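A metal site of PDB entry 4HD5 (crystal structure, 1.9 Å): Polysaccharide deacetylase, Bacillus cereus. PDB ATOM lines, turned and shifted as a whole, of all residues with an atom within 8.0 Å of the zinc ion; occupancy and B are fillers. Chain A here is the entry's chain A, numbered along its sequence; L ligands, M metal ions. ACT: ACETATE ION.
The zinc ion is bound by the side-chain carboxylate (OD1) of Asp 206 (2.0 Å), a ring nitrogen (NE2) of His 264 (2.2 Å), an oxygen (OXT) of the ligand (2.2 Å) and a ring nitrogen (NE2) of His 268 (2.3 Å).
Slightly farther from the zinc ion lies an oxygen (O) of the ligand (2.7 Å).
PXU 302 touches the zinc ion.
Four residues have an atom within 4 Å of the zinc ion: Asp 206, His 264, His 268 and PXU 302.
Along chain A the residues within 4 Å of the zinc ion span positions 206 to 302.
N of Ile 235 is in hydrogen-bond range of O of Asp 206, at 3.2 Å.
N of Asp 206 lies within hydrogen-bond range of O of Tyr 233, 2.7 Å away.
A ring nitrogen (NE2) of His 264 lies close to OA of PXU 302.
The backbone carbonyl oxygen (O) of Ala 300 sits at hydrogen-bond distance from a ring nitrogen (ND1) of His 264.
The backbone NH of His 264 lies within hydrogen-bond range of the backbone carbonyl oxygen of Met 234, at 2.8 Å.
OA of PXU 302 sits close to a ring nitrogen (NE2) of His 268 (3.3 Å).
N of His 268 sits at hydrogen-bond distance from OG1 of Thr 265, at 2.8 Å.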
ATOM      1  N   MET A 148     -35.692  -8.163   1.271  1.00  0.00           N
ATOM      2  CA  MET A 148     -35.025  -8.628   0.066  1.00  0.00           C
ATOM      3  C   MET A 148     -35.880  -9.729  -0.560  1.00  0.00           C
ATOM      4  O   MET A 148     -36.003 -10.808   0.000  1.00  0.00           O
ATOM      5  CB  MET A 148     -33.629  -9.177   0.381  1.00  0.00           C
ATOM      6  CG  MET A 148     -32.914  -9.773  -0.835  1.00  0.00           C
ATOM      7  SD  MET A 148     -31.211 -10.277  -0.482  1.00  0.00           S
ATOM      8  CE  MET A 148     -31.430 -11.280   0.962  1.00  0.00           C
ATOM      9  N   TYR A 149     -36.452  -9.420  -1.713  1.00  0.00           N
ATOM     10  CA  TYR A 149     -37.101 -10.411  -2.555  1.00  0.00           C
ATOM     11  C   TYR A 149     -36.230 -10.618  -3.783  1.00  0.00           C
ATOM     12  O   TYR A 149     -35.361  -9.783  -4.091  1.00  0.00           O
ATOM     13  CB  TYR A 149     -38.485  -9.916  -2.991  1.00  0.00           C
ATOM     14  CG  TYR A 149     -39.539  -9.908  -1.906  1.00  0.00           C
ATOM     15  CD1 TYR A 149     -40.275 -11.050  -1.610  1.00  0.00           C
ATOM     16  CD2 TYR A 149     -39.845  -8.738  -1.221  1.00  0.00           C
ATOM     17  CE1 TYR A 149     -41.254 -11.033  -0.636  1.00  0.00           C
ATOM     18  CE2 TYR A 149     -40.819  -8.708  -0.256  1.00  0.00           C
ATOM     19  CZ  TYR A 149     -41.520  -9.856   0.048  1.00  0.00           C
ATOM     20  OH  TYR A 149     -42.487  -9.825   1.007  1.00  0.00           O
ATOM     21  N   HIS A 150     -36.447 -11.708  -4.486  1.00  0.00           N
ATOM     22  CA  HIS A 150     -35.864 -11.886  -5.804  1.00  0.00           C
ATOM     23  C   HIS A 150     -36.966 -12.142  -6.821  1.00  0.00           C
ATOM     24  O   HIS A 150     -37.442 -11.196  -7.428  1.00  0.00           O
ATOM     25  CB  HIS A 150     -34.838 -13.022  -5.799  1.00  0.00           C
ATOM     26  CG  HIS A 150     -33.496 -12.613  -5.299  1.00  0.00           C
ATOM     27  ND1 HIS A 150     -33.208 -12.541  -3.957  1.00  0.00           N
ATOM     28  CD2 HIS A 150     -32.363 -12.289  -5.952  1.00  0.00           C
ATOM     29  CE1 HIS A 150     -31.952 -12.173  -3.800  1.00  0.00           C
ATOM     30  NE2 HIS A 150     -31.410 -12.018  -4.991  1.00  0.00           N
ATOM     31  N   LEU A 163     -35.157 -18.629  -3.637  1.00  0.00           N
ATOM     32  CA  LEU A 163     -35.314 -17.263  -4.141  1.00  0.00           C
ATOM     33  C   LEU A 163     -36.690 -16.978  -4.764  1.00  0.00           C
ATOM     34  O   LEU A 163     -36.946 -15.870  -5.232  1.00  0.00           O
ATOM     35  CB  LEU A 163     -34.213 -16.935  -5.181  1.00  0.00           C
ATOM     36  CG  LEU A 163     -32.896 -16.288  -4.715  1.00  0.00           C
ATOM     37  CD1 LEU A 163     -32.470 -16.729  -3.325  1.00  0.00           C
ATOM     38  CD2 LEU A 163     -31.785 -16.528  -5.729  1.00  0.00           C
ATOM     39  N   PHE A 204     -36.315  -5.674  -4.618  1.00  0.00           N
ATOM     40  CA  PHE A 204     -36.211  -6.832  -5.506  1.00  0.00           C
ATOM     41  C   PHE A 204     -34.862  -6.789  -6.197  1.00  0.00           C
ATOM     42  O   PHE A 204     -34.487  -5.753  -6.709  1.00  0.00           O
ATOM     43  CB  PHE A 204     -37.294  -6.813  -6.599  1.00  0.00           C
ATOM     44  CG  PHE A 204     -38.703  -6.813  -6.073  1.00  0.00           C
ATOM     45  CD1 PHE A 204     -39.340  -5.630  -5.760  1.00  0.00           C
ATOM     46  CD2 PHE A 204     -39.378  -7.998  -5.890  1.00  0.00           C
ATOM     47  CE1 PHE A 204     -40.628  -5.629  -5.266  1.00  0.00           C
ATOM     48  CE2 PHE A 204     -40.665  -8.016  -5.381  1.00  0.00           C
ATOM     49  CZ  PHE A 204     -41.297  -6.819  -5.076  1.00  0.00           C
ATOM     50  N   ASP A 205     -34.128  -7.897  -6.199  1.00  0.00           N
ATOM     51  CA  ASP A 205     -32.830  -7.948  -6.874  1.00  0.00           C
ATOM     52  C   ASP A 205     -32.910  -8.621  -8.242  1.00  0.00           C
ATOM     53  O   ASP A 205     -33.468  -9.703  -8.357  1.00  0.00           O
ATOM     54  CB  ASP A 205     -31.805  -8.683  -6.009  1.00  0.00           C
ATOM     55  CG  ASP A 205     -31.373  -7.886  -4.787  1.00  0.00           C
ATOM     56  OD1 ASP A 205     -31.972  -6.838  -4.495  1.00  0.00           O
ATOM     57  OD2 ASP A 205     -30.455  -8.325  -4.088  1.00  0.00           O
ATOM     58  N   ASP A 206     -32.359  -7.932  -9.248  1.00  0.00           N
ATOM     59  CA  ASP A 206     -31.925  -8.499 -10.560  1.00  0.00           C
ATOM     60  C   ASP A 206     -32.674  -7.969 -11.780  1.00  0.00           C
ATOM     61  O   ASP A 206     -32.058  -7.796 -12.847  1.00  0.00           O
ATOM     62  CB  ASP A 206     -31.944 -10.040 -10.589  1.00  0.00           C
ATOM     63  CG  ASP A 206     -30.885 -10.646  -9.728  1.00  0.00           C
ATOM     64  OD1 ASP A 206     -30.102  -9.911  -9.086  1.00  0.00           O
ATOM     65  OD2 ASP A 206     -30.811 -11.895  -9.710  1.00  0.00           O
ATOM     66  N   GLY A 207     -33.973  -7.699 -11.630  1.00  0.00           N
ATOM     67  CA  GLY A 207     -34.773  -7.198 -12.745  1.00  0.00           C
ATOM     68  C   GLY A 207     -35.386  -8.293 -13.595  1.00  0.00           C
ATOM     69  O   GLY A 207     -35.453  -8.177 -14.825  1.00  0.00           O
ATOM     70  N   TYR A 233     -33.711  -3.473  -8.050  1.00  0.00           N
ATOM     71  CA  TYR A 233     -32.302  -3.332  -8.424  1.00  0.00           C
ATOM     72  C   TYR A 233     -32.018  -4.049  -9.738  1.00  0.00           C
ATOM     73  O   TYR A 233     -31.983  -5.272  -9.791  1.00  0.00           O
ATOM     74  CB  TYR A 233     -31.405  -3.894  -7.339  1.00  0.00           C
ATOM     75  CG  TYR A 233     -31.481  -3.189  -6.006  1.00  0.00           C
ATOM     76  CD1 TYR A 233     -30.930  -1.937  -5.821  1.00  0.00           C
ATOM     77  CD2 TYR A 233     -32.063  -3.811  -4.914  1.00  0.00           C
ATOM     78  CE1 TYR A 233     -30.967  -1.315  -4.595  1.00  0.00           C
ATOM     79  CE2 TYR A 233     -32.111  -3.198  -3.685  1.00  0.00           C
ATOM     80  CZ  TYR A 233     -31.549  -1.954  -3.518  1.00  0.00           C
ATOM     81  OH  TYR A 233     -31.588  -1.360  -2.281  1.00  0.00           O
ATOM     82  N   MET A 234     -31.812  -3.285 -10.806  1.00  0.00           N
ATOM     83  CA  MET A 234     -31.664  -3.840 -12.146  1.00  0.00           C
ATOM     84  C   MET A 234     -30.217  -4.129 -12.564  1.00  0.00           C
ATOM     85  O   MET A 234     -29.334  -3.297 -12.371  1.00  0.00           O
ATOM     86  CB  MET A 234     -32.255  -2.850 -13.156  1.00  0.00           C
ATOM     87  CG  MET A 234     -32.319  -3.375 -14.576  1.00  0.00           C
ATOM     88  SD  MET A 234     -33.660  -4.547 -14.801  1.00  0.00           S
ATOM     89  CE  MET A 234     -33.086  -5.418 -16.263  1.00  0.00           C
ATOM     90  N   ILE A 235     -29.992  -5.309 -13.131  1.00  0.00           N
ATOM     91  CA  ILE A 235     -28.732  -5.594 -13.824  1.00  0.00           C
ATOM     92  C   ILE A 235     -28.814  -4.820 -15.143  1.00  0.00           C
ATOM     93  O   ILE A 235     -29.541  -5.218 -16.054  1.00  0.00           O
ATOM     94  CB  ILE A 235     -28.508  -7.089 -14.091  1.00  0.00           C
ATOM     95  CG1 ILE A 235     -28.423  -7.877 -12.769  1.00  0.00           C
ATOM     96  CG2 ILE A 235     -27.235  -7.289 -14.900  1.00  0.00           C
ATOM     97  CD1 ILE A 235     -28.426  -9.381 -12.942  1.00  0.00           C
ATOM     98  N   HIS A 264     -27.954  -2.521 -10.010  1.00  0.00           N
ATOM     99  CA  HIS A 264     -27.412  -3.773  -9.532  1.00  0.00           C
ATOM    100  C   HIS A 264     -26.069  -4.083 -10.194  1.00  0.00           C
ATOM    101  O   HIS A 264     -25.699  -5.251 -10.355  1.00  0.00           O
ATOM    102  CB  HIS A 264     -28.423  -4.891  -9.782  1.00  0.00           C
ATOM    103  CG  HIS A 264     -28.331  -6.012  -8.814  1.00  0.00           C
ATOM    104  ND1 HIS A 264     -27.738  -5.883  -7.583  1.00  0.00           N
ATOM    105  CD2 HIS A 264     -28.766  -7.292  -8.889  1.00  0.00           C
ATOM    106  CE1 HIS A 264     -27.813  -7.025  -6.928  1.00  0.00           C
ATOM    107  NE2 HIS A 264     -28.420  -7.897  -7.708  1.00  0.00           N
ATOM    108  N   THR A 265     -25.337  -3.011 -10.511  1.00  0.00           N
ATOM    109  CA  THR A 265     -24.184  -2.998 -11.399  1.00  0.00           C
ATOM    110  C   THR A 265     -24.602  -3.257 -12.857  1.00  0.00           C
ATOM    111  O   THR A 265     -25.793  -3.519 -13.148  1.00  0.00           O
ATOM    112  CB  THR A 265     -23.058  -3.986 -10.990  1.00  0.00           C
ATOM    113  OG1 THR A 265     -23.407  -5.318 -11.385  1.00  0.00           O
ATOM    114  CG2 THR A 265     -22.801  -3.916  -9.491  1.00  0.00           C
ATOM    115  N   HIS A 268     -23.643  -7.511 -13.137  1.00  0.00           N
ATOM    116  CA  HIS A 268     -23.744  -8.353 -11.943  1.00  0.00           C
ATOM    117  C   HIS A 268     -22.340  -8.814 -11.545  1.00  0.00           C
ATOM    118  O   HIS A 268     -22.099  -9.990 -11.299  1.00  0.00           O
ATOM    119  CB  HIS A 268     -24.711  -9.535 -12.192  1.00  0.00           C
ATOM    120  CG  HIS A 268     -25.377 -10.039 -10.952  1.00  0.00           C
ATOM    121  ND1 HIS A 268     -25.256 -11.352 -10.532  1.00  0.00           N
ATOM    122  CD2 HIS A 268     -26.166  -9.419 -10.052  1.00  0.00           C
ATOM    123  CE1 HIS A 268     -25.956 -11.512  -9.422  1.00  0.00           C
ATOM    124  NE2 HIS A 268     -26.531 -10.363  -9.115  1.00  0.00           N
ATOM    125  N   ALA A 300     -27.449  -2.417  -4.948  1.00  0.00           N
ATOM    126  CA  ALA A 300     -27.292  -3.627  -4.149  1.00  0.00           C
ATOM    127  C   ALA A 300     -26.051  -4.338  -4.667  1.00  0.00           C
ATOM    128  O   ALA A 300     -25.895  -4.536  -5.872  1.00  0.00           O
ATOM    129  CB  ALA A 300     -28.527  -4.515  -4.267  1.00  0.00           C
ATOM    130  N   TYR A 301     -25.185  -4.742  -3.743  1.00  0.00           N
ATOM    131  CA  TYR A 301     -23.949  -5.446  -4.120  1.00  0.00           C
ATOM    132  C   TYR A 301     -24.266  -6.863  -4.586  1.00  0.00           C
ATOM    133  O   TYR A 301     -24.833  -7.639  -3.834  1.00  0.00           O
ATOM    134  CB  TYR A 301     -23.002  -5.532  -2.939  1.00  0.00           C
ATOM    135  CG  TYR A 301     -22.601  -4.212  -2.312  1.00  0.00           C
ATOM    136  CD1 TYR A 301     -21.836  -3.284  -3.008  1.00  0.00           C
ATOM    137  CD2 TYR A 301     -22.948  -3.915  -1.002  1.00  0.00           C
ATOM    138  CE1 TYR A 301     -21.439  -2.086  -2.417  1.00  0.00           C
ATOM    139  CE2 TYR A 301     -22.565  -2.718  -0.397  1.00  0.00           C
ATOM    140  CZ  TYR A 301     -21.819  -1.796  -1.114  1.00  0.00           C
ATOM    141  OH  TYR A 301     -21.421  -0.615  -0.538  1.00  0.00           O
ATOM    142  N   PXU A 302     -23.869  -7.219  -5.814  1.00  0.00           N
ATOM    143  CA  PXU A 302     -24.048  -8.593  -6.292  1.00  0.00           C
ATOM    144  OA  PXU A 302     -25.431  -8.908  -6.350  1.00  0.00           O
ATOM    145  CB  PXU A 302     -23.440  -8.654  -7.681  1.00  0.00           C
ATOM    146  CG  PXU A 302     -23.455  -7.216  -8.161  1.00  0.00           C
ATOM    147  CD  PXU A 302     -23.294  -6.400  -6.894  1.00  0.00           C
ATOM    148  C   PXU A 302     -23.424  -9.605  -5.365  1.00  0.00           C
ATOM    149  O   PXU A 302     -22.344  -9.349  -4.812  1.00  0.00           O
ATOM    150  N   PHE A 303     -24.123 -10.719  -5.162  1.00  0.00           N
ATOM    151  CA  PHE A 303     -23.695 -11.823  -4.272  1.00  0.00           C
ATOM    152  C   PHE A 303     -23.574 -11.411  -2.807  1.00  0.00           C
ATOM    153  O   PHE A 303     -23.098 -12.189  -1.976  1.00  0.00           O
ATOM    154  CB  PHE A 303     -22.363 -12.441  -4.764  1.00  0.00           C
ATOM    155  CG  PHE A 303     -22.302 -12.671  -6.247  1.00  0.00           C
ATOM    156  CD1 PHE A 303     -22.939 -13.764  -6.829  1.00  0.00           C
ATOM    157  CD2 PHE A 303     -21.600 -11.794  -7.057  1.00  0.00           C
ATOM    158  CE1 PHE A 303     -22.882 -13.962  -8.200  1.00  0.00           C
ATOM    159  CE2 PHE A 303     -21.550 -11.987  -8.434  1.00  0.00           C
ATOM    160  CZ  PHE A 303     -22.177 -13.076  -9.006  1.00  0.00           C
ATOM    161  N   GLY A 304     -23.984 -10.189  -2.498  1.00  0.00           N
ATOM    162  CA  GLY A 304     -23.654  -9.567  -1.215  1.00  0.00           C
ATOM    163  C   GLY A 304     -22.178  -9.331  -0.941  1.00  0.00           C
ATOM    164  O   GLY A 304     -21.818  -9.027   0.190  1.00  0.00           O
ATOM    165  N   THR A 324     -26.390  -8.436   1.659  1.00  0.00           N
ATOM    166  CA  THR A 324     -27.288  -9.542   1.942  1.00  0.00           C
ATOM    167  C   THR A 324     -27.172  -9.991   3.394  1.00  0.00           C
ATOM    168  O   THR A 324     -27.752 -11.012   3.772  1.00  0.00           O
ATOM    169  CB  THR A 324     -27.029 -10.726   1.000  1.00  0.00           C
ATOM    170  OG1 THR A 324     -25.715 -11.240   1.212  1.00  0.00           O
ATOM    171  CG2 THR A 324     -27.162 -10.285  -0.441  1.00  0.00           C
ATOM    172  N   ARG A 343     -30.294  -6.475   5.161  1.00  0.00           N
ATOM    173  CA  ARG A 343     -31.625  -6.718   4.647  1.00  0.00           C
ATOM    174  C   ARG A 343     -32.234  -7.963   5.283  1.00  0.00           C
ATOM    175  O   ARG A 343     -31.516  -8.857   5.770  1.00  0.00           O
ATOM    176  CB  ARG A 343     -31.594  -6.827   3.133  1.00  0.00           C
ATOM    177  CG  ARG A 343     -31.395  -5.495   2.441  1.00  0.00           C
ATOM    178  CD  ARG A 343     -31.748  -5.563   0.970  1.00  0.00           C
ATOM    179  NE  ARG A 343     -30.723  -6.294   0.204  1.00  0.00           N
ATOM    180  CZ  ARG A 343     -30.807  -6.571  -1.100  1.00  0.00           C
ATOM    181  NH1 ARG A 343     -31.881  -6.202  -1.792  1.00  0.00           N
ATOM    182  NH2 ARG A 343     -29.824  -7.232  -1.704  1.00  0.00           N
HETATM  183  C   ACT L   1     -27.830 -11.254  -5.421  1.00  0.00           C
HETATM  184  O   ACT L   1     -26.798 -11.170  -6.101  1.00  0.00           O
HETATM  185  OXT ACT L   1     -28.969 -11.039  -5.923  1.00  0.00           O
HETATM  186  CH3 ACT L   1     -27.693 -11.627  -3.974  1.00  0.00           C
HETATM  187 ZN    ZN M   1     -28.506 -10.105  -7.915  1.00  0.00          ZN
